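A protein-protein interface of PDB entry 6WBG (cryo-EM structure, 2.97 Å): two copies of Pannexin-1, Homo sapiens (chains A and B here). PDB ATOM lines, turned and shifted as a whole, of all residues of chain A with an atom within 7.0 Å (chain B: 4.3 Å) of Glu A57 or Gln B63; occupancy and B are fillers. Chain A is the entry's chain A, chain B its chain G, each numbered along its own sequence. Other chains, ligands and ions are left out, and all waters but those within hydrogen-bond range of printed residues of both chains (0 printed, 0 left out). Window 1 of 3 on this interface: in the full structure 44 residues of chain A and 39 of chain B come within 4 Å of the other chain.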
ATOM      1  N   ALA A   2      20.179   2.100  37.024  1.00  0.00           N
ATOM      2  CA  ALA A   2      18.812   2.518  36.753  1.00  0.00           C
ATOM      3  C   ALA A   2      18.787   3.869  36.060  1.00  0.00           C
ATOM      4  O   ALA A   2      19.656   4.706  36.285  1.00  0.00           O
ATOM      5  CB  ALA A   2      18.010   2.570  38.039  1.00  0.00           C
ATOM      6  N   ILE A   3      17.777   4.072  35.214  1.00  0.00           N
ATOM      7  CA  ILE A   3      17.634   5.337  34.499  1.00  0.00           C
ATOM      8  C   ILE A   3      17.506   6.501  35.469  1.00  0.00           C
ATOM      9  O   ILE A   3      18.149   7.544  35.299  1.00  0.00           O
ATOM     10  CB  ILE A   3      16.439   5.262  33.534  1.00  0.00           C
ATOM     11  CG1 ILE A   3      16.887   4.743  32.170  1.00  0.00           C
ATOM     12  CG2 ILE A   3      15.764   6.598  33.392  1.00  0.00           C
ATOM     13  CD1 ILE A   3      17.758   5.694  31.431  1.00  0.00           C
ATOM     14  N   ALA A   4      16.675   6.349  36.499  1.00  0.00           N
ATOM     15  CA  ALA A   4      16.424   7.466  37.400  1.00  0.00           C
ATOM     16  C   ALA A   4      17.666   7.815  38.209  1.00  0.00           C
ATOM     17  O   ALA A   4      17.883   8.983  38.549  1.00  0.00           O
ATOM     18  CB  ALA A   4      15.249   7.139  38.313  1.00  0.00           C
ATOM     19  N   PHE A  54      23.423   2.170  27.811  1.00  0.00           N
ATOM     20  CA  PHE A  54      23.581   0.853  28.408  1.00  0.00           C
ATOM     21  C   PHE A  54      22.772   0.701  29.685  1.00  0.00           C
ATOM     22  O   PHE A  54      23.117  -0.123  30.537  1.00  0.00           O
ATOM     23  CB  PHE A  54      25.056   0.574  28.662  1.00  0.00           C
ATOM     24  CG  PHE A  54      25.897   0.734  27.445  1.00  0.00           C
ATOM     25  CD1 PHE A  54      25.876  -0.222  26.451  1.00  0.00           C
ATOM     26  CD2 PHE A  54      26.676   1.853  27.274  1.00  0.00           C
ATOM     27  CE1 PHE A  54      26.633  -0.072  25.320  1.00  0.00           C
ATOM     28  CE2 PHE A  54      27.434   2.007  26.149  1.00  0.00           C
ATOM     29  CZ  PHE A  54      27.414   1.041  25.171  1.00  0.00           C
ATOM     30  N   ALA A  55      21.720   1.496  29.843  1.00  0.00           N
ATOM     31  CA  ALA A  55      20.778   1.269  30.924  1.00  0.00           C
ATOM     32  C   ALA A  55      20.284  -0.168  30.869  1.00  0.00           C
ATOM     33  O   ALA A  55      20.024  -0.711  29.793  1.00  0.00           O
ATOM     34  CB  ALA A  55      19.604   2.239  30.825  1.00  0.00           C
ATOM     35  N   GLN A  56      20.164  -0.791  32.042  1.00  0.00           N
ATOM     36  CA  GLN A  56      19.918  -2.227  32.087  1.00  0.00           C
ATOM     37  C   GLN A  56      18.602  -2.604  31.419  1.00  0.00           C
ATOM     38  O   GLN A  56      18.403  -3.768  31.056  1.00  0.00           O
ATOM     39  CB  GLN A  56      19.939  -2.713  33.534  1.00  0.00           C
ATOM     40  CG  GLN A  56      20.052  -4.219  33.670  1.00  0.00           C
ATOM     41  CD  GLN A  56      21.187  -4.784  32.843  1.00  0.00           C
ATOM     42  OE1 GLN A  56      20.967  -5.356  31.777  1.00  0.00           O
ATOM     43  NE2 GLN A  56      22.412  -4.622  33.331  1.00  0.00           N
ATOM     44  N   GLU A  57      17.697  -1.645  31.241  1.00  0.00           N
ATOM     45  CA  GLU A  57      16.408  -1.967  30.640  1.00  0.00           C
ATOM     46  C   GLU A  57      16.384  -1.659  29.149  1.00  0.00           C
ATOM     47  O   GLU A  57      15.476  -2.092  28.435  1.00  0.00           O
ATOM     48  CB  GLU A  57      15.291  -1.223  31.356  1.00  0.00           C
ATOM     49  CG  GLU A  57      15.344   0.269  31.242  1.00  0.00           C
ATOM     50  CD  GLU A  57      16.096   0.886  32.389  1.00  0.00           C
ATOM     51  OE1 GLU A  57      16.908   0.182  33.023  1.00  0.00           O
ATOM     52  OE2 GLU A  57      15.836   2.061  32.696  1.00  0.00           O
ATOM     53  N   ILE A  58      17.357  -0.895  28.662  1.00  0.00           N
ATOM     54  CA  ILE A  58      17.434  -0.670  27.224  1.00  0.00           C
ATOM     55  C   ILE A  58      18.364  -1.690  26.583  1.00  0.00           C
ATOM     56  O   ILE A  58      18.180  -2.077  25.424  1.00  0.00           O
ATOM     57  CB  ILE A  58      17.863   0.777  26.941  1.00  0.00           C
ATOM     58  CG1 ILE A  58      16.782   1.731  27.428  1.00  0.00           C
ATOM     59  CG2 ILE A  58      18.052   0.999  25.470  1.00  0.00           C
ATOM     60  CD1 ILE A  58      15.498   1.625  26.642  1.00  0.00           C
ATOM     61  N   SER A  59      19.354  -2.162  27.331  1.00  0.00           N
ATOM     62  CA  SER A  59      20.252  -3.206  26.852  1.00  0.00           C
ATOM     63  C   SER A  59      19.543  -4.549  26.939  1.00  0.00           C
ATOM     64  O   SER A  59      19.037  -4.925  28.000  1.00  0.00           O
ATOM     65  CB  SER A  59      21.542  -3.213  27.665  1.00  0.00           C
ATOM     66  OG  SER A  59      22.256  -2.005  27.487  1.00  0.00           O
ATOM     67  N   ILE A  60      19.503  -5.278  25.824  1.00  0.00           N
ATOM     68  CA  ILE A  60      18.915  -6.611  25.839  1.00  0.00           C
ATOM     69  C   ILE A  60      19.910  -7.625  26.381  1.00  0.00           C
ATOM     70  O   ILE A  60      19.526  -8.661  26.935  1.00  0.00           O
ATOM     71  CB  ILE A  60      18.423  -6.996  24.432  1.00  0.00           C
ATOM     72  CG1 ILE A  60      17.613  -8.288  24.486  1.00  0.00           C
ATOM     73  CG2 ILE A  60      19.593  -7.153  23.484  1.00  0.00           C
ATOM     74  CD1 ILE A  60      16.533  -8.274  25.529  1.00  0.00           C
ATOM     75  N   GLY A  61      21.199  -7.342  26.246  1.00  0.00           N
ATOM     76  CA  GLY A  61      22.220  -8.291  26.632  1.00  0.00           C
ATOM     77  C   GLY A  61      23.574  -7.905  26.085  1.00  0.00           C
ATOM     78  O   GLY A  61      24.040  -6.782  26.298  1.00  0.00           O
ATOM     79  N   PHE B  54      10.655  -1.165  36.000  1.00  0.00           N
ATOM     80  CA  PHE B  54      11.682  -2.192  35.957  1.00  0.00           C
ATOM     81  C   PHE B  54      12.072  -2.673  37.344  1.00  0.00           C
ATOM     82  O   PHE B  54      13.185  -3.170  37.531  1.00  0.00           O
ATOM     83  CB  PHE B  54      12.899  -1.678  35.197  1.00  0.00           C
ATOM     84  CG  PHE B  54      12.565  -1.170  33.838  1.00  0.00           C
ATOM     85  CD1 PHE B  54      12.283  -2.050  32.816  1.00  0.00           C
ATOM     86  CD2 PHE B  54      12.493   0.180  33.595  1.00  0.00           C
ATOM     87  CE1 PHE B  54      11.958  -1.591  31.568  1.00  0.00           C
ATOM     88  CE2 PHE B  54      12.170   0.644  32.350  1.00  0.00           C
ATOM     89  CZ  PHE B  54      11.904  -0.243  31.334  1.00  0.00           C
ATOM     90  N   GLY B  61      12.069 -10.558  33.243  1.00  0.00           N
ATOM     91  CA  GLY B  61      13.355 -10.845  32.646  1.00  0.00           C
ATOM     92  C   GLY B  61      13.696  -9.854  31.559  1.00  0.00           C
ATOM     93  O   GLY B  61      13.679  -8.641  31.785  1.00  0.00           O
ATOM     94  N   THR B  62      14.017 -10.360  30.373  1.00  0.00           N
ATOM     95  CA  THR B  62      14.321  -9.487  29.250  1.00  0.00           C
ATOM     96  C   THR B  62      13.108  -8.645  28.882  1.00  0.00           C
ATOM     97  O   THR B  62      11.979  -8.922  29.292  1.00  0.00           O
ATOM     98  CB  THR B  62      14.770 -10.305  28.042  1.00  0.00           C
ATOM     99  OG1 THR B  62      13.724 -11.207  27.664  1.00  0.00           O
ATOM    100  CG2 THR B  62      16.023 -11.096  28.371  1.00  0.00           C
ATOM    101  N   GLN B  63      13.356  -7.597  28.094  1.00  0.00           N
ATOM    102  CA  GLN B  63      12.277  -6.710  27.687  1.00  0.00           C
ATOM    103  C   GLN B  63      11.584  -7.219  26.435  1.00  0.00           C
ATOM    104  O   GLN B  63      10.511  -6.722  26.077  1.00  0.00           O
ATOM    105  CB  GLN B  63      12.813  -5.302  27.459  1.00  0.00           C
ATOM    106  CG  GLN B  63      13.657  -4.785  28.601  1.00  0.00           C
ATOM    107  CD  GLN B  63      15.113  -5.163  28.449  1.00  0.00           C
ATOM    108  OE1 GLN B  63      15.545  -5.583  27.379  1.00  0.00           O
ATOM    109  NE2 GLN B  63      15.872  -5.033  29.526  1.00  0.00           N
ATOM    110  N   ILE B  64      12.178  -8.189  25.750  1.00  0.00           N
ATOM    111  CA  ILE B  64      11.623  -8.739  24.522  1.00  0.00           C
ATOM    112  C   ILE B  64      11.835 -10.246  24.532  1.00  0.00           C
ATOM    113  O   ILE B  64      12.827 -10.736  25.079  1.00  0.00           O
ATOM    114  CB  ILE B  64      12.264  -8.100  23.279  1.00  0.00           C
ATOM    115  CG1 ILE B  64      11.585  -8.586  22.005  1.00  0.00           C
ATOM    116  CG2 ILE B  64      13.740  -8.407  23.222  1.00  0.00           C
ATOM    117  CD1 ILE B  64      12.138  -7.961  20.762  1.00  0.00           C
ATOM    118  N   TRP B  85      15.058  -6.955  18.939  1.00  0.00           N
ATOM    119  CA  TRP B  85      15.171  -5.792  19.811  1.00  0.00           C
ATOM    120  C   TRP B  85      15.842  -4.634  19.092  1.00  0.00           C
ATOM    121  O   TRP B  85      15.372  -3.495  19.153  1.00  0.00           O
ATOM    122  CB  TRP B  85      15.950  -6.166  21.067  1.00  0.00           C
ATOM    123  CG  TRP B  85      16.107  -5.054  22.036  1.00  0.00           C
ATOM    124  CD1 TRP B  85      17.262  -4.433  22.382  1.00  0.00           C
ATOM    125  CD2 TRP B  85      15.072  -4.434  22.800  1.00  0.00           C
ATOM    126  NE1 TRP B  85      17.016  -3.461  23.314  1.00  0.00           N
ATOM    127  CE2 TRP B  85      15.675  -3.442  23.587  1.00  0.00           C
ATOM    128  CE3 TRP B  85      13.696  -4.619  22.894  1.00  0.00           C
ATOM    129  CZ2 TRP B  85      14.952  -2.640  24.453  1.00  0.00           C
ATOM    130  CZ3 TRP B  85      12.979  -3.822  23.753  1.00  0.00           C
ATOM    131  CH2 TRP B  85      13.607  -2.846  24.522  1.00  0.00           C
ATOM    132  N   PRO B 110      11.153   4.450  28.629  1.00  0.00           N
ATOM    133  CA  PRO B 110      11.919   5.047  29.732  1.00  0.00           C
ATOM    134  C   PRO B 110      12.664   6.297  29.321  1.00  0.00           C
ATOM    135  O   PRO B 110      12.731   7.260  30.093  1.00  0.00           O
ATOM    136  CB  PRO B 110      12.884   3.925  30.135  1.00  0.00           C
ATOM    137  CG  PRO B 110      12.289   2.699  29.602  1.00  0.00           C
ATOM    138  CD  PRO B 110      11.597   3.076  28.352  1.00  0.00           C
ATOM    139  N   LYS B 266       7.368 -10.412  21.201  1.00  0.00           N
ATOM    140  CA  LYS B 266       6.502  -9.620  22.061  1.00  0.00           C
ATOM    141  C   LYS B 266       7.356  -8.775  22.988  1.00  0.00           C
ATOM    142  O   LYS B 266       8.306  -9.279  23.592  1.00  0.00           O
ATOM    143  CB  LYS B 266       5.565 -10.494  22.892  1.00  0.00           C
ATOM    144  CG  LYS B 266       4.592  -9.684  23.723  1.00  0.00           C
ATOM    145  CD  LYS B 266       3.602 -10.566  24.438  1.00  0.00           C
ATOM    146  CE  LYS B 266       2.573  -9.741  25.176  1.00  0.00           C
ATOM    147  NZ  LYS B 266       1.675  -9.033  24.235  1.00  0.00           N
ATOM    148  N   LEU B 267       7.017  -7.498  23.096  1.00  0.00           N
ATOM    149  CA  LEU B 267       7.730  -6.596  23.991  1.00  0.00           C
ATOM    150  C   LEU B 267       7.113  -6.719  25.373  1.00  0.00           C
ATOM    151  O   LEU B 267       6.061  -6.145  25.650  1.00  0.00           O
ATOM    152  CB  LEU B 267       7.669  -5.166  23.479  1.00  0.00           C
ATOM    153  CG  LEU B 267       8.497  -4.896  22.232  1.00  0.00           C
ATOM    154  CD1 LEU B 267       8.188  -3.525  21.718  1.00  0.00           C
ATOM    155  CD2 LEU B 267       9.965  -5.017  22.544  1.00  0.00           C
ATOM    156  N   ILE B 268       7.765  -7.487  26.241  1.00  0.00           N
ATOM    157  CA  ILE B 268       7.323  -7.582  27.621  1.00  0.00           C
ATOM    158  C   ILE B 268       7.411  -6.205  28.264  1.00  0.00           C
ATOM    159  O   ILE B 268       8.109  -5.307  27.772  1.00  0.00           O
ATOM    160  CB  ILE B 268       8.162  -8.611  28.395  1.00  0.00           C
ATOM    161  CG1 ILE B 268       8.490  -9.807  27.508  1.00  0.00           C
ATOM    162  CG2 ILE B 268       7.420  -9.094  29.618  1.00  0.00           C
ATOM    163  CD1 ILE B 268       7.279 -10.557  27.028  1.00  0.00           C
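Positions printed for both chains: 54 and 61.
Printed residues of chain A that touch a printed residue of chain B: Gln A56, Glu A57, Ile A58, Ser A59 and Ile A60. Hydrophobic or aromatic side chains of chain A within 4 Å of the printed part of chain B: Ile A60. Of the 10 printed residues of chain B, 5 touch a printed residue of chain A. Printed residues of chain B that touch a printed residue of chain A: Phe B54, Thr B62, Gln B63, Ile B64 and Trp B85. Hydrophobic or aromatic side chains of chain B within 4 Å of the printed part of chain A: Phe B54, Ile B64 and Trp B85. Among the printed residues, 9 pairs touch across the chains.
O of Ala A55 is in hydrogen-bond range of OG of Ser A59 (3.5 Å). The backbone carbonyl oxygen of Ile B64 sits at hydrogen-bond distance from the side-chain hydroxyl of Thr B62, 2.8 Å away. The backbone NH of Ile B268 lies within hydrogen-bond range of the backbone carbonyl oxygen of Gln B63 (2.9 Å).
Glu A57 touches Phe B54. Gln B63 touches Ser A59 (NE2 to O, 3.5 Å). CB of Thr B62 touches CD1 of Ile A60, at 3.7 Å. Gln B63 touches Ile A60. CD1 of Ile A60 touches CG2 of Ile B64, at 3.6 Å. Trp B85 touches Ile A60 (CD1 to CB, 3.5 Å).
Glu A57 touches just these residues of chain B: Phe B54 (3.4 Å) and Gln B63 (3.1 Å). Of the printed residues of chain B, Ile A58 touches Trp B85 (2.8 Å). Of the printed residues of chain B, Ile A60 touches Thr B62, Gln B63, Ile B64 and Trp B85. Gln B63 touches four residues of chain A. Pro B110 touches none of the printed residues of chain A. Lys B266 touches none of the printed residues of chain A. The nearest residue of chain A that does not touch Gln B63 is Ile A58 (4.5 Å).
The side-chain amide nitrogen (NE2) of Gln B63 lies within hydrogen-bond range of the backbone carbonyl oxygen (O) of Gln A56 (3.2 Å). The backbone carbonyl oxygen of Glu A57 lies close to the side-chain amide nitrogen of Gln B63 (3.2 Å). The indole nitrogen of Trp B85 is in hydrogen-bond range of the backbone carbonyl oxygen of Ile A58, 2.8 Å away.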
